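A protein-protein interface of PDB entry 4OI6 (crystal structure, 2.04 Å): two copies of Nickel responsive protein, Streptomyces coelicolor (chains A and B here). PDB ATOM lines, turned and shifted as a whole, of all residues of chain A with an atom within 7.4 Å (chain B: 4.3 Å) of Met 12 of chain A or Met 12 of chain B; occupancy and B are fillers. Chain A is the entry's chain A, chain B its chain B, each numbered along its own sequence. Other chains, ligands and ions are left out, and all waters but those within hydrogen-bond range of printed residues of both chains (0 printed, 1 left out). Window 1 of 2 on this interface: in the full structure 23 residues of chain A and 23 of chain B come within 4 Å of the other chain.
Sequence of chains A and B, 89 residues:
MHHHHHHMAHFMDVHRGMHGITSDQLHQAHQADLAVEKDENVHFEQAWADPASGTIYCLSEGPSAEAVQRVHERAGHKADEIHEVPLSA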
ATOM      1  N   HIS A  10     -13.864  20.252 -35.082  1.00  0.00           N
ATOM      2  CA  HIS A  10     -14.186  20.957 -33.829  1.00  0.00           C
ATOM      3  C   HIS A  10     -13.047  20.922 -32.797  1.00  0.00           C
ATOM      4  O   HIS A  10     -12.356  19.903 -32.648  1.00  0.00           O
ATOM      5  CB  HIS A  10     -15.479  20.411 -33.218  1.00  0.00           C
ATOM      6  CG  HIS A  10     -16.709  20.835 -33.948  1.00  0.00           C
ATOM      7  ND1 HIS A  10     -17.217  20.138 -35.030  1.00  0.00           N
ATOM      8  CD2 HIS A  10     -17.527  21.903 -33.777  1.00  0.00           C
ATOM      9  CE1 HIS A  10     -18.294  20.751 -35.478  1.00  0.00           C
ATOM     10  NE2 HIS A  10     -18.505  21.828 -34.738  1.00  0.00           N
ATOM     11  N   PHE A  11     -12.860  22.044 -32.094  1.00  0.00           N
ATOM     12  CA  PHE A  11     -11.778  22.187 -31.114  1.00  0.00           C
ATOM     13  C   PHE A  11     -12.229  22.801 -29.794  1.00  0.00           C
ATOM     14  O   PHE A  11     -13.104  23.669 -29.761  1.00  0.00           O
ATOM     15  CB  PHE A  11     -10.645  23.040 -31.698  1.00  0.00           C
ATOM     16  CG  PHE A  11     -10.064  22.462 -32.949  1.00  0.00           C
ATOM     17  CD1 PHE A  11     -10.575  22.816 -34.188  1.00  0.00           C
ATOM     18  CD2 PHE A  11      -9.046  21.518 -32.884  1.00  0.00           C
ATOM     19  CE1 PHE A  11     -10.062  22.260 -35.344  1.00  0.00           C
ATOM     20  CE2 PHE A  11      -8.523  20.957 -34.044  1.00  0.00           C
ATOM     21  CZ  PHE A  11      -9.034  21.324 -35.264  1.00  0.00           C
ATOM     22  N   MET A  12     -11.607  22.347 -28.710  1.00  0.00           N
ATOM     23  CA  MET A  12     -11.797  22.952 -27.404  1.00  0.00           C
ATOM     24  C   MET A  12     -10.439  23.438 -26.954  1.00  0.00           C
ATOM     25  O   MET A  12      -9.491  22.652 -26.894  1.00  0.00           O
ATOM     26  CB  MET A  12     -12.316  21.926 -26.398  1.00  0.00           C
ATOM     27  CG  MET A  12     -12.545  22.523 -25.004  1.00  0.00           C
ATOM     28  SD  MET A  12     -14.221  23.541 -25.007  1.00  0.00           S
ATOM     29  CE  MET A  12     -15.434  22.051 -24.747  1.00  0.00           C
ATOM     30  N   ASP A  13     -10.330  24.731 -26.661  1.00  0.00           N
ATOM     31  CA  ASP A  13      -9.073  25.278 -26.180  1.00  0.00           C
ATOM     32  C   ASP A  13      -9.247  25.880 -24.790  1.00  0.00           C
ATOM     33  O   ASP A  13     -10.359  26.209 -24.378  1.00  0.00           O
ATOM     34  CB  ASP A  13      -8.461  26.281 -27.184  1.00  0.00           C
ATOM     35  CG  ASP A  13      -9.250  27.584 -27.297  1.00  0.00           C
ATOM     36  OD1 ASP A  13      -9.518  28.240 -26.267  1.00  0.00           O
ATOM     37  OD2 ASP A  13      -9.593  27.961 -28.433  1.00  0.00           O
ATOM     38  N   VAL A  14      -8.139  25.994 -24.066  1.00  0.00           N
ATOM     39  CA  VAL A  14      -8.128  26.458 -22.685  1.00  0.00           C
ATOM     40  C   VAL A  14      -7.080  27.544 -22.502  1.00  0.00           C
ATOM     41  O   VAL A  14      -5.908  27.377 -22.942  1.00  0.00           O
ATOM     42  CB  VAL A  14      -7.758  25.334 -21.719  1.00  0.00           C
ATOM     43  CG1 VAL A  14      -7.977  25.794 -20.281  1.00  0.00           C
ATOM     44  CG2 VAL A  14      -8.566  24.085 -22.002  1.00  0.00           C
ATOM     45  N   GLN A  46     -18.566  28.859 -28.821  1.00  0.00           N
ATOM     46  CA  GLN A  46     -18.930  29.166 -27.447  1.00  0.00           C
ATOM     47  C   GLN A  46     -17.692  29.466 -26.635  1.00  0.00           C
ATOM     48  O   GLN A  46     -16.630  28.892 -26.875  1.00  0.00           O
ATOM     49  CB  GLN A  46     -19.744  28.019 -26.821  1.00  0.00           C
ATOM     50  CG  GLN A  46     -21.289  28.166 -26.874  1.00  0.00           C
ATOM     51  CD  GLN A  46     -21.849  29.139 -25.827  1.00  0.00           C
ATOM     52  OE1 GLN A  46     -21.275  30.195 -25.559  1.00  0.00           O
ATOM     53  NE2 GLN A  46     -22.978  28.774 -25.231  1.00  0.00           N
ATOM     54  N   ALA A  47     -17.828  30.401 -25.699  1.00  0.00           N
ATOM     55  CA  ALA A  47     -16.762  30.676 -24.750  1.00  0.00           C
ATOM     56  C   ALA A  47     -17.343  30.718 -23.342  1.00  0.00           C
ATOM     57  O   ALA A  47     -18.329  31.423 -23.084  1.00  0.00           O
ATOM     58  CB  ALA A  47     -16.082  31.971 -25.085  1.00  0.00           C
ATOM     59  N   TRP A  48     -16.740  29.958 -22.433  1.00  0.00           N
ATOM     60  CA  TRP A  48     -17.159  29.971 -21.042  1.00  0.00           C
ATOM     61  C   TRP A  48     -15.966  30.344 -20.174  1.00  0.00           C
ATOM     62  O   TRP A  48     -14.859  29.895 -20.442  1.00  0.00           O
ATOM     63  CB  TRP A  48     -17.631  28.584 -20.624  1.00  0.00           C
ATOM     64  CG  TRP A  48     -18.713  27.990 -21.476  1.00  0.00           C
ATOM     65  CD1 TRP A  48     -20.073  28.112 -21.304  1.00  0.00           C
ATOM     66  CD2 TRP A  48     -18.522  27.130 -22.610  1.00  0.00           C
ATOM     67  NE1 TRP A  48     -20.730  27.394 -22.284  1.00  0.00           N
ATOM     68  CE2 TRP A  48     -19.810  26.783 -23.084  1.00  0.00           C
ATOM     69  CE3 TRP A  48     -17.393  26.638 -23.269  1.00  0.00           C
ATOM     70  CZ2 TRP A  48     -19.983  25.943 -24.207  1.00  0.00           C
ATOM     71  CZ3 TRP A  48     -17.569  25.803 -24.383  1.00  0.00           C
ATOM     72  CH2 TRP A  48     -18.856  25.465 -24.835  1.00  0.00           C
ATOM     73  N   ILE A  56     -10.583  29.766 -18.949  1.00  0.00           N
ATOM     74  CA  ILE A  56     -11.501  29.995 -20.061  1.00  0.00           C
ATOM     75  C   ILE A  56     -11.489  28.799 -21.007  1.00  0.00           C
ATOM     76  O   ILE A  56     -10.411  28.329 -21.406  1.00  0.00           O
ATOM     77  CB  ILE A  56     -11.151  31.260 -20.864  1.00  0.00           C
ATOM     78  CG1 ILE A  56     -11.036  32.479 -19.947  1.00  0.00           C
ATOM     79  CG2 ILE A  56     -12.197  31.510 -21.964  1.00  0.00           C
ATOM     80  CD1 ILE A  56     -10.728  33.762 -20.696  1.00  0.00           C
ATOM     81  N   TYR A  57     -12.682  28.319 -21.360  1.00  0.00           N
ATOM     82  CA  TYR A  57     -12.859  27.266 -22.368  1.00  0.00           C
ATOM     83  C   TYR A  57     -13.491  27.821 -23.639  1.00  0.00           C
ATOM     84  O   TYR A  57     -14.537  28.458 -23.583  1.00  0.00           O
ATOM     85  CB  TYR A  57     -13.766  26.162 -21.819  1.00  0.00           C
ATOM     86  CG  TYR A  57     -13.189  25.427 -20.631  1.00  0.00           C
ATOM     87  CD1 TYR A  57     -13.589  25.731 -19.332  1.00  0.00           C
ATOM     88  CD2 TYR A  57     -12.243  24.428 -20.813  1.00  0.00           C
ATOM     89  CE1 TYR A  57     -13.053  25.046 -18.242  1.00  0.00           C
ATOM     90  CE2 TYR A  57     -11.703  23.745 -19.738  1.00  0.00           C
ATOM     91  CZ  TYR A  57     -12.108  24.059 -18.460  1.00  0.00           C
ATOM     92  OH  TYR A  57     -11.556  23.367 -17.410  1.00  0.00           O
ATOM     93  N   CYS A  58     -12.872  27.567 -24.788  1.00  0.00           N
ATOM     94  CA  CYS A  58     -13.442  27.996 -26.065  1.00  0.00           C
ATOM     95  C   CYS A  58     -13.685  26.817 -27.008  1.00  0.00           C
ATOM     96  O   CYS A  58     -12.766  26.069 -27.356  1.00  0.00           O
ATOM     97  CB  CYS A  58     -12.561  29.052 -26.758  1.00  0.00           C
ATOM     98  SG  CYS A  58     -12.428  30.662 -25.907  1.00  0.00           S
ATOM     99  N   LEU A  59     -14.946  26.662 -27.403  1.00  0.00           N
ATOM    100  CA  LEU A  59     -15.343  25.714 -28.425  1.00  0.00           C
ATOM    101  C   LEU A  59     -15.384  26.449 -29.760  1.00  0.00           C
ATOM    102  O   LEU A  59     -16.084  27.475 -29.918  1.00  0.00           O
ATOM    103  CB  LEU A  59     -16.734  25.143 -28.124  1.00  0.00           C
ATOM    104  CG  LEU A  59     -17.239  24.215 -29.238  1.00  0.00           C
ATOM    105  CD1 LEU A  59     -16.461  22.887 -29.236  1.00  0.00           C
ATOM    106  CD2 LEU A  59     -18.736  23.963 -29.113  1.00  0.00           C
ATOM    107  N   SER A  60     -14.635  25.919 -30.722  1.00  0.00           N
ATOM    108  CA  SER A  60     -14.576  26.499 -32.056  1.00  0.00           C
ATOM    109  C   SER A  60     -14.773  25.439 -33.120  1.00  0.00           C
ATOM    110  O   SER A  60     -14.599  24.238 -32.868  1.00  0.00           O
ATOM    111  CB  SER A  60     -13.222  27.180 -32.286  1.00  0.00           C
ATOM    112  OG  SER A  60     -12.169  26.228 -32.341  1.00  0.00           O
ATOM    113  N   VAL A  68      -6.781  27.732 -35.557  1.00  0.00           N
ATOM    114  CA  VAL A  68      -7.399  28.304 -34.368  1.00  0.00           C
ATOM    115  C   VAL A  68      -6.369  29.101 -33.576  1.00  0.00           C
ATOM    116  O   VAL A  68      -6.619  30.241 -33.148  1.00  0.00           O
ATOM    117  CB  VAL A  68      -7.988  27.210 -33.468  1.00  0.00           C
ATOM    118  CG1 VAL A  68      -8.569  27.817 -32.185  1.00  0.00           C
ATOM    119  CG2 VAL A  68      -9.067  26.414 -34.217  1.00  0.00           C
ATOM    120  N   ALA A  79      -3.900  30.343 -26.867  1.00  0.00           N
ATOM    121  CA  ALA A  79      -4.460  29.407 -25.888  1.00  0.00           C
ATOM    122  C   ALA A  79      -3.342  28.550 -25.308  1.00  0.00           C
ATOM    123  O   ALA A  79      -2.393  28.217 -26.018  1.00  0.00           O
ATOM    124  CB  ALA A  79      -5.511  28.527 -26.538  1.00  0.00           C
ATOM    125  N   GLU A  81      -3.803  25.474 -24.150  1.00  0.00           N
ATOM    126  CA  GLU A  81      -3.992  24.159 -24.757  1.00  0.00           C
ATOM    127  C   GLU A  81      -5.081  24.202 -25.791  1.00  0.00           C
ATOM    128  O   GLU A  81      -6.043  24.940 -25.641  1.00  0.00           O
ATOM    129  CB  GLU A  81      -4.391  23.115 -23.707  1.00  0.00           C
ATOM    130  CG  GLU A  81      -3.359  22.872 -22.638  1.00  0.00           C
ATOM    131  CD  GLU A  81      -3.666  21.626 -21.845  1.00  0.00           C
ATOM    132  OE1 GLU A  81      -3.767  20.557 -22.485  1.00  0.00           O
ATOM    133  OE2 GLU A  81      -3.831  21.727 -20.604  1.00  0.00           O
ATOM    134  N   ILE A  82      -4.945  23.379 -26.820  1.00  0.00           N
ATOM    135  CA  ILE A  82      -5.998  23.217 -27.805  1.00  0.00           C
ATOM    136  C   ILE A  82      -6.094  21.752 -28.242  1.00  0.00           C
ATOM    137  O   ILE A  82      -5.090  21.130 -28.609  1.00  0.00           O
ATOM    138  CB  ILE A  82      -5.800  24.147 -29.021  1.00  0.00           C
ATOM    139  CG1 ILE A  82      -6.794  23.781 -30.109  1.00  0.00           C
ATOM    140  CG2 ILE A  82      -4.378  24.046 -29.577  1.00  0.00           C
ATOM    141  CD1 ILE A  82      -7.045  24.904 -31.043  1.00  0.00           C
ATOM    142  N   HIS A  83      -7.304  21.202 -28.177  1.00  0.00           N
ATOM    143  CA  HIS A  83      -7.527  19.795 -28.492  1.00  0.00           C
ATOM    144  C   HIS A  83      -8.664  19.641 -29.490  1.00  0.00           C
ATOM    145  O   HIS A  83      -9.677  20.319 -29.369  1.00  0.00           O
ATOM    146  CB  HIS A  83      -7.892  19.030 -27.214  1.00  0.00           C
ATOM    147  CG  HIS A  83      -6.801  19.003 -26.188  1.00  0.00           C
ATOM    148  ND1 HIS A  83      -5.791  18.065 -26.195  1.00  0.00           N
ATOM    149  CD2 HIS A  83      -6.569  19.792 -25.110  1.00  0.00           C
ATOM    150  CE1 HIS A  83      -4.981  18.282 -25.176  1.00  0.00           C
ATOM    151  NE2 HIS A  83      -5.431  19.320 -24.499  1.00  0.00           N
ATOM    152  N   GLU A  84      -8.517  18.752 -30.468  1.00  0.00           N
ATOM    153  CA  GLU A  84      -9.633  18.508 -31.378  1.00  0.00           C
ATOM    154  C   GLU A  84     -10.658  17.649 -30.647  1.00  0.00           C
ATOM    155  O   GLU A  84     -10.294  16.690 -29.960  1.00  0.00           O
ATOM    156  CB  GLU A  84      -9.170  17.796 -32.655  1.00  0.00           C
ATOM    157  CG  GLU A  84     -10.188  17.853 -33.809  1.00  0.00           C
ATOM    158  CD  GLU A  84      -9.720  17.090 -35.048  1.00  0.00           C
ATOM    159  OE1 GLU A  84      -8.494  16.971 -35.243  1.00  0.00           O
ATOM    160  OE2 GLU A  84     -10.572  16.603 -35.823  1.00  0.00           O
ATOM    161  N   VAL A  85     -11.934  17.983 -30.795  1.00  0.00           N
ATOM    162  CA  VAL A  85     -12.998  17.160 -30.223  1.00  0.00           C
ATOM    163  C   VAL A  85     -13.895  16.599 -31.335  1.00  0.00           C
ATOM    164  O   VAL A  85     -14.999  17.093 -31.564  1.00  0.00           O
ATOM    165  CB  VAL A  85     -13.817  17.941 -29.151  1.00  0.00           C
ATOM    166  CG1 VAL A  85     -13.011  18.077 -27.858  1.00  0.00           C
ATOM    167  CG2 VAL A  85     -14.199  19.334 -29.661  1.00  0.00           C
ATOM    168  N   PHE B  11     -21.526  24.575 -15.348  1.00  0.00           N
ATOM    169  CA  PHE B  11     -20.248  23.944 -15.016  1.00  0.00           C
ATOM    170  C   PHE B  11     -19.623  23.282 -16.242  1.00  0.00           C
ATOM    171  O   PHE B  11     -20.330  22.741 -17.104  1.00  0.00           O
ATOM    172  CB  PHE B  11     -20.443  22.909 -13.891  1.00  0.00           C
ATOM    173  CG  PHE B  11     -21.134  23.478 -12.675  1.00  0.00           C
ATOM    174  CD1 PHE B  11     -22.526  23.515 -12.602  1.00  0.00           C
ATOM    175  CD2 PHE B  11     -20.392  24.003 -11.626  1.00  0.00           C
ATOM    176  CE1 PHE B  11     -23.165  24.066 -11.501  1.00  0.00           C
ATOM    177  CE2 PHE B  11     -21.029  24.563 -10.517  1.00  0.00           C
ATOM    178  CZ  PHE B  11     -22.411  24.588 -10.456  1.00  0.00           C
ATOM    179  N   MET B  12     -18.295  23.365 -16.329  1.00  0.00           N
ATOM    180  CA  MET B  12     -17.543  22.580 -17.301  1.00  0.00           C
ATOM    181  C   MET B  12     -16.759  21.585 -16.473  1.00  0.00           C
ATOM    182  O   MET B  12     -16.053  21.969 -15.529  1.00  0.00           O
ATOM    183  CB  MET B  12     -16.577  23.455 -18.114  1.00  0.00           C
ATOM    184  CG  MET B  12     -15.780  22.663 -19.179  1.00  0.00           C
ATOM    185  SD  MET B  12     -16.954  22.066 -20.658  1.00  0.00           S
ATOM    186  CE  MET B  12     -17.088  23.772 -21.616  1.00  0.00           C
ATOM    187  N   ASP B  13     -16.903  20.306 -16.790  1.00  0.00           N
ATOM    188  CA  ASP B  13     -16.139  19.294 -16.091  1.00  0.00           C
ATOM    189  C   ASP B  13     -15.338  18.454 -17.078  1.00  0.00           C
ATOM    190  O   ASP B  13     -15.679  18.351 -18.255  1.00  0.00           O
ATOM    191  CB  ASP B  13     -17.020  18.447 -15.140  1.00  0.00           C
ATOM    192  CG  ASP B  13     -17.909  17.429 -15.871  1.00  0.00           C
ATOM    193  OD1 ASP B  13     -17.382  16.552 -16.608  1.00  0.00           O
ATOM    194  OD2 ASP B  13     -19.146  17.493 -15.679  1.00  0.00           O
ATOM    195  N   TRP B  48     -18.237  16.668 -25.338  1.00  0.00           N
ATOM    196  CA  TRP B  48     -17.333  16.606 -26.481  1.00  0.00           C
ATOM    197  C   TRP B  48     -16.199  15.705 -26.064  1.00  0.00           C
ATOM    198  O   TRP B  48     -15.801  15.730 -24.913  1.00  0.00           O
ATOM    199  CB  TRP B  48     -16.752  17.991 -26.782  1.00  0.00           C
ATOM    200  CG  TRP B  48     -17.778  19.058 -27.057  1.00  0.00           C
ATOM    201  CD1 TRP B  48     -18.287  19.419 -28.279  1.00  0.00           C
ATOM    202  CD2 TRP B  48     -18.415  19.909 -26.090  1.00  0.00           C
ATOM    203  NE1 TRP B  48     -19.197  20.446 -28.126  1.00  0.00           N
ATOM    204  CE2 TRP B  48     -19.293  20.768 -26.795  1.00  0.00           C
ATOM    205  CE3 TRP B  48     -18.326  20.033 -24.699  1.00  0.00           C
ATOM    206  CZ2 TRP B  48     -20.083  21.727 -26.152  1.00  0.00           C
ATOM    207  CZ3 TRP B  48     -19.103  20.990 -24.064  1.00  0.00           C
ATOM    208  CH2 TRP B  48     -19.970  21.825 -24.789  1.00  0.00           C
ATOM    209  N   TYR B  57     -15.071  16.399 -22.245  1.00  0.00           N
ATOM    210  CA  TYR B  57     -15.529  17.684 -21.720  1.00  0.00           C
ATOM    211  C   TYR B  57     -17.050  17.647 -21.588  1.00  0.00           C
ATOM    212  O   TYR B  57     -17.756  17.247 -22.516  1.00  0.00           O
ATOM    213  CB  TYR B  57     -15.127  18.818 -22.670  1.00  0.00           C
ATOM    214  CG  TYR B  57     -13.636  18.915 -22.950  1.00  0.00           C
ATOM    215  CD1 TYR B  57     -13.051  18.180 -23.971  1.00  0.00           C
ATOM    216  CD2 TYR B  57     -12.825  19.755 -22.196  1.00  0.00           C
ATOM    217  CE1 TYR B  57     -11.684  18.271 -24.231  1.00  0.00           C
ATOM    218  CE2 TYR B  57     -11.457  19.861 -22.446  1.00  0.00           C
ATOM    219  CZ  TYR B  57     -10.891  19.119 -23.461  1.00  0.00           C
ATOM    220  OH  TYR B  57      -9.529  19.218 -23.706  1.00  0.00           O
ATOM    221  N   CYS B  58     -17.553  18.050 -20.426  1.00  0.00           N
ATOM    222  CA  CYS B  58     -18.989  18.049 -20.166  1.00  0.00           C
ATOM    223  C   CYS B  58     -19.476  19.428 -19.724  1.00  0.00           C
ATOM    224  O   CYS B  58     -18.992  19.978 -18.733  1.00  0.00           O
ATOM    225  CB  CYS B  58     -19.341  17.020 -19.084  1.00  0.00           C
ATOM    226  SG  CYS B  58     -19.449  15.296 -19.640  1.00  0.00           S
ATOM    227  N   LEU B  59     -20.438  19.982 -20.459  1.00  0.00           N
ATOM    228  CA  LEU B  59     -21.111  21.214 -20.044  1.00  0.00           C
ATOM    229  C   LEU B  59     -22.464  20.860 -19.441  1.00  0.00           C
ATOM    230  O   LEU B  59     -23.282  20.162 -20.082  1.00  0.00           O
ATOM    231  CB  LEU B  59     -21.333  22.144 -21.234  1.00  0.00           C
ATOM    232  CG  LEU B  59     -22.145  23.391 -20.921  1.00  0.00           C
ATOM    233  CD1 LEU B  59     -21.329  24.342 -20.061  1.00  0.00           C
ATOM    234  CD2 LEU B  59     -22.600  24.081 -22.194  1.00  0.00           C
ATOM    235  N   ILE B  82     -13.658  19.963 -12.185  1.00  0.00           N
ATOM    236  CA  ILE B  82     -14.905  20.686 -12.458  1.00  0.00           C
ATOM    237  C   ILE B  82     -14.818  22.157 -12.050  1.00  0.00           C
ATOM    238  O   ILE B  82     -14.337  22.478 -10.961  1.00  0.00           O
ATOM    239  CB  ILE B  82     -16.151  20.005 -11.808  1.00  0.00           C
ATOM    240  CG1 ILE B  82     -17.425  20.780 -12.171  1.00  0.00           C
ATOM    241  CG2 ILE B  82     -15.988  19.873 -10.301  1.00  0.00           C
ATOM    242  CD1 ILE B  82     -18.694  20.048 -11.856  1.00  0.00           C
ATOM    243  N   HIS B  83     -15.266  23.046 -12.933  1.00  0.00           N
ATOM    244  CA  HIS B  83     -15.263  24.478 -12.634  1.00  0.00           C
ATOM    245  C   HIS B  83     -16.636  25.076 -12.943  1.00  0.00           C
ATOM    246  O   HIS B  83     -17.233  24.767 -13.982  1.00  0.00           O
ATOM    247  CB  HIS B  83     -14.185  25.199 -13.457  1.00  0.00           C
ATOM    248  CG  HIS B  83     -12.801  24.654 -13.265  1.00  0.00           C
ATOM    249  ND1 HIS B  83     -12.063  24.883 -12.123  1.00  0.00           N
ATOM    250  CD2 HIS B  83     -12.024  23.888 -14.067  1.00  0.00           C
ATOM    251  CE1 HIS B  83     -10.890  24.283 -12.232  1.00  0.00           C
ATOM    252  NE2 HIS B  83     -10.842  23.670 -13.404  1.00  0.00           N
ATOM    253  N   VAL B  85     -18.809  27.894 -14.448  1.00  0.00           N
ATOM    254  CA  VAL B  85     -18.542  28.900 -15.485  1.00  0.00           C
ATOM    255  C   VAL B  85     -19.689  29.917 -15.568  1.00  0.00           C
ATOM    256  O   VAL B  85     -20.556  29.820 -16.430  1.00  0.00           O
ATOM    257  CB  VAL B  85     -18.213  28.267 -16.884  1.00  0.00           C
ATOM    258  CG1 VAL B  85     -16.846  27.586 -16.866  1.00  0.00           C
ATOM    259  CG2 VAL B  85     -19.276  27.256 -17.311  1.00  0.00           C
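The backbone carbonyl oxygen (O) of Trp 48 of chain B sits at hydrogen-bond distance from the backbone NH (N) of Tyr 57 of chain B, at 2.8 Å. OE1 of Glu 81 of chain A lies close to NE2 of His 83 of chain A, at 2.9 Å. The backbone carbonyl oxygen of His 10 of chain A lies within hydrogen-bond range of the backbone NH of Val 85 of chain A (2.7 Å). The backbone NH (N) of Tyr 57 of chain A sits at hydrogen-bond distance from the backbone carbonyl oxygen (O) of Trp 48 of chain A. The backbone carbonyl oxygen (O) of His 83 of chain A is in hydrogen-bond range of the backbone NH (N) of Met 12 of chain A (2.9 Å). The backbone carbonyl oxygen (O) of Met 12 of chain B sits at hydrogen-bond distance from the backbone NH (N) of His 83 of chain B, at 2.9 Å.
Of the 20 printed residues of chain A, 6 touch a printed residue of chain B. Of the 10 printed residues of chain B, 6 touch a printed residue of chain A. Hydrophobic or aromatic side chains of chain B that line the printed part of chain A: Met 12, Trp 48, Tyr 57, Leu 59, His 83 and Val 85. Among the printed residues, 13 pairs touch across the chains. Among the printed residues, no Asp or Glu carboxylate lies within 4 Å of a Lys or Arg side-chain nitrogen of the other chain.
Met 12 of chain A touches Trp 48 of chain B, and with the chains exchanged Trp 48 of chain A touches Met 12 of chain B. Met 12 of chain A touches Tyr 57 of chain B, and with the chains exchanged Tyr 57 of chain A touches Met 12 of chain B. Trp 48 of chain B touches its own counterpart, Trp 48 of chain A. Val 85 of chain A touches Tyr 57 of chain B, but with the chains exchanged Tyr 57 of chain A does not touch Val 85 of chain B (4.5 Å). Positions printed for both chains: 11, 12, 13, 48, 57, 58, 59, 82, 83 and 85.
Among the printed residues, pairs that only touch across the chains: Met 12 of chain A with Met 12 of chain B, Met 12 of chain A with Trp 48 of chain B, Met 12 of chain A with Tyr 57 of chain B, Trp 48 of chain A with Met 12 of chain B, Trp 48 of chain A with Trp 48 of chain B, Trp 48 of chain A with Leu 59 of chain B, Trp 48 of chain A with Val 85 of chain B, Tyr 57 of chain A with Met 12 of chain B, Tyr 57 of chain A with His 83 of chain B, Leu 59 of chain A with Trp 48 of chain B, His 83 of chain A with Tyr 57 of chain B, Val 85 of chain A with Trp 48 of chain B and Val 85 of chain A with Tyr 57 of chain B.
Of chain B, only Met 12 (3.9 Å), Trp 48 (3.5 Å) and Tyr 57 (3.8 Å) come within 4 Å of Met 12 of chain A. Of the printed residues of chain A, Met 12 of chain B touches Met 12, Trp 48 and Tyr 57. Of the printed residues of chain A, Trp 48 of chain B touches Met 12, Trp 48, Leu 59 and Val 85. Of the printed residues of chain B, Tyr 57 of chain A touches Met 12 and His 83. Of the printed residues of chain B, Trp 48 of chain A touches Met 12, Trp 48, Leu 59 and Val 85.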
